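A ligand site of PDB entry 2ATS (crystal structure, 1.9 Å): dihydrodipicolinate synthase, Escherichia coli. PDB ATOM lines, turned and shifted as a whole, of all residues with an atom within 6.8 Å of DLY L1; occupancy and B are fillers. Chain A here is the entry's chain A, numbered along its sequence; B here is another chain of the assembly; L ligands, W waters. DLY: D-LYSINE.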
ATOM      1  N   VAL A  42      25.734  -8.026  17.603  1.00  0.00           N
ATOM      2  CA  VAL A  42      24.938  -7.279  16.618  1.00  0.00           C
ATOM      3  C   VAL A  42      23.442  -7.448  16.874  1.00  0.00           C
ATOM      4  O   VAL A  42      22.684  -7.798  15.993  1.00  0.00           O
ATOM      5  CB  VAL A  42      25.310  -7.604  15.130  1.00  0.00           C
ATOM      6  CG1 VAL A  42      24.639  -6.604  14.191  1.00  0.00           C
ATOM      7  CG2 VAL A  42      26.819  -7.536  14.921  1.00  0.00           C
ATOM      8  N   GLU A  47      23.965  -1.854  16.938  1.00  0.00           N
ATOM      9  CA  GLU A  47      23.636  -1.137  15.701  1.00  0.00           C
ATOM     10  C   GLU A  47      23.348  -2.055  14.496  1.00  0.00           C
ATOM     11  O   GLU A  47      23.843  -1.843  13.388  1.00  0.00           O
ATOM     12  CB  GLU A  47      24.727  -0.097  15.387  1.00  0.00           C
ATOM     13  CG  GLU A  47      24.610   1.146  16.259  1.00  0.00           C
ATOM     14  CD  GLU A  47      25.817   2.050  16.150  1.00  0.00           C
ATOM     15  OE1 GLU A  47      26.797   1.811  16.927  1.00  0.00           O
ATOM     16  OE2 GLU A  47      25.783   2.986  15.328  1.00  0.00           O
ATOM     17  N   SER A  48      22.574  -3.094  14.741  1.00  0.00           N
ATOM     18  CA  SER A  48      22.163  -4.008  13.684  1.00  0.00           C
ATOM     19  C   SER A  48      21.536  -3.302  12.469  1.00  0.00           C
ATOM     20  O   SER A  48      21.817  -3.678  11.334  1.00  0.00           O
ATOM     21  CB  SER A  48      21.189  -5.034  14.232  1.00  0.00           C
ATOM     22  OG  SER A  48      20.085  -4.374  14.802  1.00  0.00           O
ATOM     23  N   ALA A  49      20.698  -2.286  12.710  1.00  0.00           N
ATOM     24  CA  ALA A  49      20.005  -1.570  11.618  1.00  0.00           C
ATOM     25  C   ALA A  49      20.949  -1.001  10.565  1.00  0.00           C
ATOM     26  O   ALA A  49      20.631  -1.029   9.378  1.00  0.00           O
ATOM     27  CB  ALA A  49      19.155  -0.445  12.187  1.00  0.00           C
ATOM     28  N   THR A  50      22.069  -0.426  11.014  1.00  0.00           N
ATOM     29  CA  THR A  50      22.979   0.327  10.144  1.00  0.00           C
ATOM     30  C   THR A  50      24.207  -0.438   9.622  1.00  0.00           C
ATOM     31  O   THR A  50      24.995   0.129   8.899  1.00  0.00           O
ATOM     32  CB  THR A  50      23.474   1.630  10.827  1.00  0.00           C
ATOM     33  OG1 THR A  50      24.049   1.332  12.099  1.00  0.00           O
ATOM     34  CG2 THR A  50      22.274   2.604  11.128  1.00  0.00           C
ATOM     35  N   LEU A  51      24.327  -1.715   9.995  1.00  0.00           N
ATOM     36  CA  LEU A  51      25.305  -2.607   9.364  1.00  0.00           C
ATOM     37  C   LEU A  51      24.610  -3.362   8.245  1.00  0.00           C
ATOM     38  O   LEU A  51      23.502  -3.892   8.431  1.00  0.00           O
ATOM     39  CB  LEU A  51      25.849  -3.593  10.399  1.00  0.00           C
ATOM     40  CG  LEU A  51      26.569  -2.958  11.610  1.00  0.00           C
ATOM     41  CD1 LEU A  51      26.835  -3.973  12.691  1.00  0.00           C
ATOM     42  CD2 LEU A  51      27.860  -2.299  11.170  1.00  0.00           C
ATOM     43  N   ASN A  52      25.267  -3.451   7.107  1.00  0.00           N
ATOM     44  CA  ASN A  52      24.709  -4.277   6.043  1.00  0.00           C
ATOM     45  C   ASN A  52      24.906  -5.754   6.372  1.00  0.00           C
ATOM     46  O   ASN A  52      25.617  -6.093   7.339  1.00  0.00           O
ATOM     47  CB  ASN A  52      25.199  -3.878   4.653  1.00  0.00           C
ATOM     48  CG  ASN A  52      26.664  -4.177   4.412  1.00  0.00           C
ATOM     49  OD1 ASN A  52      27.193  -5.220   4.824  1.00  0.00           O
ATOM     50  ND2 ASN A  52      27.324  -3.285   3.689  1.00  0.00           N
ATOM     51  N   HIS A  53      24.276  -6.622   5.601  1.00  0.00           N
ATOM     52  CA  HIS A  53      24.273  -8.061   5.954  1.00  0.00           C
ATOM     53  C   HIS A  53      25.690  -8.633   6.084  1.00  0.00           C
ATOM     54  O   HIS A  53      25.969  -9.415   6.990  1.00  0.00           O
ATOM     55  CB  HIS A  53      23.423  -8.871   4.969  1.00  0.00           C
ATOM     56  CG  HIS A  53      21.951  -8.713   5.179  1.00  0.00           C
ATOM     57  ND1 HIS A  53      21.255  -9.438   6.128  1.00  0.00           N
ATOM     58  CD2 HIS A  53      21.043  -7.890   4.598  1.00  0.00           C
ATOM     59  CE1 HIS A  53      19.986  -9.070   6.125  1.00  0.00           C
ATOM     60  NE2 HIS A  53      19.826  -8.137   5.199  1.00  0.00           N
ATOM     61  N   ASP A  54      26.588  -8.241   5.175  1.00  0.00           N
ATOM     62  CA  ASP A  54      27.963  -8.707   5.254  1.00  0.00           C
ATOM     63  C   ASP A  54      28.718  -8.109   6.413  1.00  0.00           C
ATOM     64  O   ASP A  54      29.459  -8.817   7.123  1.00  0.00           O
ATOM     65  CB  ASP A  54      28.715  -8.411   3.968  1.00  0.00           C
ATOM     66  CG  ASP A  54      28.203  -9.196   2.801  1.00  0.00           C
ATOM     67  OD1 ASP A  54      27.947 -10.407   2.932  1.00  0.00           O
ATOM     68  OD2 ASP A  54      28.036  -8.688   1.682  1.00  0.00           O
ATOM     69  N   HIS A  56      27.469  -7.069   9.148  1.00  0.00           N
ATOM     70  CA  HIS A  56      26.821  -7.684  10.310  1.00  0.00           C
ATOM     71  C   HIS A  56      27.466  -9.067  10.580  1.00  0.00           C
ATOM     72  O   HIS A  56      27.939  -9.329  11.694  1.00  0.00           O
ATOM     73  CB  HIS A  56      25.333  -7.794   9.978  1.00  0.00           C
ATOM     74  CG  HIS A  56      24.469  -8.380  11.051  1.00  0.00           C
ATOM     75  ND1 HIS A  56      23.172  -7.952  11.250  1.00  0.00           N
ATOM     76  CD2 HIS A  56      24.667  -9.411  11.915  1.00  0.00           C
ATOM     77  CE1 HIS A  56      22.623  -8.667  12.212  1.00  0.00           C
ATOM     78  NE2 HIS A  56      23.508  -9.547  12.647  1.00  0.00           N
ATOM     79  N   GLY A  78      17.627 -10.981  13.781  1.00  0.00           N
ATOM     80  CA  GLY A  78      16.300 -10.456  13.505  1.00  0.00           C
ATOM     81  C   GLY A  78      16.242  -9.776  12.149  1.00  0.00           C
ATOM     82  O   GLY A  78      17.226  -9.208  11.660  1.00  0.00           O
ATOM     83  N   ALA A  79      15.077  -9.870  11.524  1.00  0.00           N
ATOM     84  CA  ALA A  79      14.794  -9.095  10.313  1.00  0.00           C
ATOM     85  C   ALA A  79      13.279  -8.992  10.161  1.00  0.00           C
ATOM     86  O   ALA A  79      12.508  -9.834  10.713  1.00  0.00           O
ATOM     87  CB  ALA A  79      15.442  -9.742   9.094  1.00  0.00           C
ATOM     88  N   ASN A  80      12.801  -7.967   9.463  1.00  0.00           N
ATOM     89  CA  ASN A  80      11.365  -7.804   9.310  1.00  0.00           C
ATOM     90  C   ASN A  80      10.849  -8.425   8.027  1.00  0.00           C
ATOM     91  O   ASN A  80       9.663  -8.380   7.775  1.00  0.00           O
ATOM     92  CB  ASN A  80      10.954  -6.332   9.406  1.00  0.00           C
ATOM     93  CG  ASN A  80      11.507  -5.486   8.262  1.00  0.00           C
ATOM     94  OD1 ASN A  80      12.410  -5.909   7.534  1.00  0.00           O
ATOM     95  ND2 ASN A  80      10.970  -4.261   8.118  1.00  0.00           N
ATOM     96  N   ALA A  81      11.733  -9.007   7.219  1.00  0.00           N
ATOM     97  CA  ALA A  81      11.340  -9.872   6.116  1.00  0.00           C
ATOM     98  C   ALA A  81      11.820 -11.275   6.484  1.00  0.00           C
ATOM     99  O   ALA A  81      12.976 -11.467   6.856  1.00  0.00           O
ATOM    100  CB  ALA A  81      11.971  -9.418   4.804  1.00  0.00           C
ATOM    101  N   GLU A  84      14.929 -12.614   4.738  1.00  0.00           N
ATOM    102  CA  GLU A  84      16.157 -12.027   5.268  1.00  0.00           C
ATOM    103  C   GLU A  84      16.610 -12.642   6.574  1.00  0.00           C
ATOM    104  O   GLU A  84      17.796 -12.822   6.805  1.00  0.00           O
ATOM    105  CB  GLU A  84      15.983 -10.525   5.557  1.00  0.00           C
ATOM    106  CG  GLU A  84      16.209  -9.623   4.381  1.00  0.00           C
ATOM    107  CD  GLU A  84      16.091  -8.158   4.783  1.00  0.00           C
ATOM    108  OE1 GLU A  84      15.138  -7.513   4.335  1.00  0.00           O
ATOM    109  OE2 GLU A  84      16.970  -7.639   5.550  1.00  0.00           O
ATOM    110  N   LEU A  88      20.205 -14.558   7.127  1.00  0.00           N
ATOM    111  CA  LEU A  88      21.102 -14.133   8.184  1.00  0.00           C
ATOM    112  C   LEU A  88      21.420 -15.321   9.083  1.00  0.00           C
ATOM    113  O   LEU A  88      22.587 -15.606   9.378  1.00  0.00           O
ATOM    114  CB  LEU A  88      20.457 -12.982   8.964  1.00  0.00           C
ATOM    115  CG  LEU A  88      21.227 -11.960   9.778  1.00  0.00           C
ATOM    116  CD1 LEU A  88      22.550 -11.522   9.150  1.00  0.00           C
ATOM    117  CD2 LEU A  88      20.295 -10.751  10.021  1.00  0.00           C
ATOM    118  N   TYR A 106       9.660  -5.457  12.506  1.00  0.00           N
ATOM    119  CA  TYR A 106       9.438  -4.031  12.802  1.00  0.00           C
ATOM    120  C   TYR A 106       8.890  -3.358  11.538  1.00  0.00           C
ATOM    121  O   TYR A 106       9.119  -3.820  10.431  1.00  0.00           O
ATOM    122  CB  TYR A 106      10.751  -3.370  13.268  1.00  0.00           C
ATOM    123  CG  TYR A 106      11.972  -3.930  12.553  1.00  0.00           C
ATOM    124  CD1 TYR A 106      12.435  -3.377  11.351  1.00  0.00           C
ATOM    125  CD2 TYR A 106      12.651  -5.049  13.072  1.00  0.00           C
ATOM    126  CE1 TYR A 106      13.517  -3.920  10.669  1.00  0.00           C
ATOM    127  CE2 TYR A 106      13.753  -5.588  12.403  1.00  0.00           C
ATOM    128  CZ  TYR A 106      14.176  -5.025  11.195  1.00  0.00           C
ATOM    129  OH  TYR A 106      15.234  -5.569  10.521  1.00  0.00           O
ATOM    130  N   HIS B  53      16.596  -4.730  -2.273  1.00  0.00           N
ATOM    131  CA  HIS B  53      16.892  -3.457  -2.908  1.00  0.00           C
ATOM    132  C   HIS B  53      16.712  -3.530  -4.429  1.00  0.00           C
ATOM    133  O   HIS B  53      16.118  -2.663  -5.035  1.00  0.00           O
ATOM    134  CB  HIS B  53      18.299  -2.967  -2.508  1.00  0.00           C
ATOM    135  CG  HIS B  53      18.314  -2.178  -1.241  1.00  0.00           C
ATOM    136  ND1 HIS B  53      18.584  -2.741  -0.002  1.00  0.00           N
ATOM    137  CD2 HIS B  53      18.059  -0.868  -1.003  1.00  0.00           C
ATOM    138  CE1 HIS B  53      18.508  -1.817   0.931  1.00  0.00           C
ATOM    139  NE2 HIS B  53      18.197  -0.665   0.353  1.00  0.00           N
ATOM    140  N   ALA B  79      14.533   4.434   4.547  1.00  0.00           N
ATOM    141  CA  ALA B  79      15.366   3.386   5.184  1.00  0.00           C
ATOM    142  C   ALA B  79      15.696   3.811   6.588  1.00  0.00           C
ATOM    143  O   ALA B  79      15.678   5.020   6.896  1.00  0.00           O
ATOM    144  CB  ALA B  79      16.646   3.153   4.386  1.00  0.00           C
ATOM    145  N   ASN B  80      15.987   2.838   7.453  1.00  0.00           N
ATOM    146  CA  ASN B  80      16.389   3.147   8.831  1.00  0.00           C
ATOM    147  C   ASN B  80      17.893   3.350   8.998  1.00  0.00           C
ATOM    148  O   ASN B  80      18.385   3.632  10.095  1.00  0.00           O
ATOM    149  CB  ASN B  80      15.823   2.134   9.846  1.00  0.00           C
ATOM    150  CG  ASN B  80      16.356   0.752   9.647  1.00  0.00           C
ATOM    151  OD1 ASN B  80      16.971   0.441   8.649  1.00  0.00           O
ATOM    152  ND2 ASN B  80      16.095  -0.107  10.620  1.00  0.00           N
ATOM    153  N   ALA B  81      18.610   3.162   7.891  1.00  0.00           N
ATOM    154  CA  ALA B  81      20.036   3.477   7.800  1.00  0.00           C
ATOM    155  C   ALA B  81      20.189   4.552   6.753  1.00  0.00           C
ATOM    156  O   ALA B  81      19.765   4.390   5.626  1.00  0.00           O
ATOM    157  CB  ALA B  81      20.851   2.214   7.410  1.00  0.00           C
ATOM    158  N   GLU B  84      21.557   3.470   3.356  1.00  0.00           N
ATOM    159  CA  GLU B  84      20.611   2.754   2.530  1.00  0.00           C
ATOM    160  C   GLU B  84      19.648   3.710   1.832  1.00  0.00           C
ATOM    161  O   GLU B  84      19.351   3.531   0.659  1.00  0.00           O
ATOM    162  CB  GLU B  84      19.807   1.770   3.353  1.00  0.00           C
ATOM    163  CG  GLU B  84      20.586   0.603   3.860  1.00  0.00           C
ATOM    164  CD  GLU B  84      19.704  -0.386   4.605  1.00  0.00           C
ATOM    165  OE1 GLU B  84      19.943  -0.593   5.808  1.00  0.00           O
ATOM    166  OE2 GLU B  84      18.748  -0.937   3.966  1.00  0.00           O
ATOM    167  N   TYR B 106      12.957   3.561  11.360  1.00  0.00           N
ATOM    168  CA  TYR B 106      12.204   2.626  12.212  1.00  0.00           C
ATOM    169  C   TYR B 106      13.143   1.709  12.993  1.00  0.00           C
ATOM    170  O   TYR B 106      14.265   1.419  12.543  1.00  0.00           O
ATOM    171  CB  TYR B 106      11.262   1.732  11.372  1.00  0.00           C
ATOM    172  CG  TYR B 106      11.819   1.371  10.019  1.00  0.00           C
ATOM    173  CD1 TYR B 106      12.561   0.203   9.842  1.00  0.00           C
ATOM    174  CD2 TYR B 106      11.670   2.213   8.915  1.00  0.00           C
ATOM    175  CE1 TYR B 106      13.102  -0.134   8.596  1.00  0.00           C
ATOM    176  CE2 TYR B 106      12.227   1.887   7.669  1.00  0.00           C
ATOM    177  CZ  TYR B 106      12.934   0.717   7.529  1.00  0.00           C
ATOM    178  OH  TYR B 106      13.480   0.390   6.313  1.00  0.00           O
ATOM    179  N   TYR B 107      12.694   1.324  14.161  1.00  0.00           N
ATOM    180  CA  TYR B 107      13.375   0.366  15.044  1.00  0.00           C
ATOM    181  C   TYR B 107      14.489   0.979  15.913  1.00  0.00           C
ATOM    182  O   TYR B 107      14.513   0.740  17.139  1.00  0.00           O
ATOM    183  CB  TYR B 107      13.844  -0.898  14.293  1.00  0.00           C
ATOM    184  CG  TYR B 107      14.382  -1.970  15.218  1.00  0.00           C
ATOM    185  CD1 TYR B 107      13.526  -2.752  15.965  1.00  0.00           C
ATOM    186  CD2 TYR B 107      15.739  -2.140  15.394  1.00  0.00           C
ATOM    187  CE1 TYR B 107      13.999  -3.735  16.819  1.00  0.00           C
ATOM    188  CE2 TYR B 107      16.231  -3.116  16.290  1.00  0.00           C
ATOM    189  CZ  TYR B 107      15.348  -3.910  16.995  1.00  0.00           C
ATOM    190  OH  TYR B 107      15.807  -4.871  17.886  1.00  0.00           O
HETATM  191  N   DLY L   1      18.519  -1.625   7.803  1.00  0.00           N
HETATM  192  CA  DLY L   1      17.776  -2.892   7.445  1.00  0.00           C
HETATM  193  C   DLY L   1      16.941  -3.373   8.598  1.00  0.00           C
HETATM  194  O   DLY L   1      17.071  -2.807   9.666  1.00  0.00           O
HETATM  195  CB  DLY L   1      18.762  -3.974   7.026  1.00  0.00           C
HETATM  196  CG  DLY L   1      19.670  -4.505   8.144  1.00  0.00           C
HETATM  197  CD  DLY L   1      20.689  -5.484   7.550  1.00  0.00           C
HETATM  198  CE  DLY L   1      21.311  -6.483   8.524  1.00  0.00           C
HETATM  199  NZ  DLY L   1      21.942  -5.834   9.662  1.00  0.00           N
HETATM  200  OXT DLY L   1      16.171  -4.354   8.489  1.00  0.00           O
HETATM  201  N   DLY L   2      13.699  -5.317   5.143  1.00  0.00           N
HETATM  202  CA  DLY L   2      14.648  -4.170   5.296  1.00  0.00           C
HETATM  203  C   DLY L   2      13.909  -2.957   5.793  1.00  0.00           C
HETATM  204  O   DLY L   2      14.526  -1.904   6.068  1.00  0.00           O
HETATM  205  CB  DLY L   2      15.386  -3.871   3.957  1.00  0.00           C
HETATM  206  CG  DLY L   2      14.484  -3.294   2.864  1.00  0.00           C
HETATM  207  CD  DLY L   2      15.096  -3.343   1.482  1.00  0.00           C
HETATM  208  CE  DLY L   2      14.522  -2.252   0.581  1.00  0.00           C
HETATM  209  NZ  DLY L   2      13.088  -2.378   0.410  1.00  0.00           N
HETATM  210  OXT DLY L   2      12.667  -2.980   5.891  1.00  0.00           O
HETATM  211  O   HOH W   1      19.378  -5.975  11.337  1.00  0.00           O
HETATM  212  O   HOH W   2      16.161  -6.789   7.749  1.00  0.00           O
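OE1 of Glu 84 of chain B is in salt-bridge range of N of DLY L1, at 2.7 Å. The backbone carbonyl oxygen (O) of Ala 49 is in hydrogen-bond range of a nitrogen (N) of DLY L1 (2.7 Å). O of Ser 48 lies within hydrogen-bond range of NZ of DLY L1 (2.7 Å). The side-chain hydroxyl of Tyr 106 of chain B lies within hydrogen-bond range of an oxygen (O) of DLY L2 (2.5 Å). The side-chain amide oxygen (OD1) of Asn 80 of chain A is in hydrogen-bond range of a nitrogen (N) of DLY L2 (2.8 Å). An oxygen (OXT) of DLY L1 lies within hydrogen-bond range of the side-chain hydroxyl (OH) of Tyr 106 of chain A, 2.5 Å away. OE1 of Glu 84 of chain A lies within salt-bridge range of N of DLY L2 (2.7 Å). A nitrogen (NZ) of DLY L1 is in hydrogen-bond range of the backbone carbonyl oxygen of Leu 51 (2.8 Å). A ring nitrogen (ND1) of His 56 sits at hydrogen-bond distance from a nitrogen (NZ) of DLY L1, 2.9 Å away. The side-chain amide oxygen (OD1) of Asn 80 of chain B is in hydrogen-bond range of a nitrogen (N) of DLY L1 (2.7 Å).
The backbone carbonyl oxygen of Tyr 106 of chain B lies within hydrogen-bond range of the side-chain amide nitrogen of Asn 80 of chain B (3.1 Å). A ring nitrogen (NE2) of His 53 of chain A is in hydrogen-bond range of the side-chain carboxylate (OE2) of Glu 84 of chain A, at 2.9 Å. O of Tyr 106 of chain A is in hydrogen-bond range of ND2 of Asn 80 of chain A (3.0 Å).
Merely in contact with DLY L1: His 53 of chain A. Hydrophobic or aromatic side chains within 4 Å of DLY L1: His 53 of chain A, His 56 and Tyr 106 of chain A.
Water W2 lies within hydrogen-bond range of the side-chain carboxylate (OE2) of Glu 84 of chain A (2.5 Å), an oxygen (OXT) of DLY L1 (2.5 Å) and the side-chain hydroxyl (OH) of Tyr 106 of chain A (3.2 Å). Water W1 lies within hydrogen-bond range of NZ of DLY L1 (3.1 Å) and O of Ser 48 (3.4 Å).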
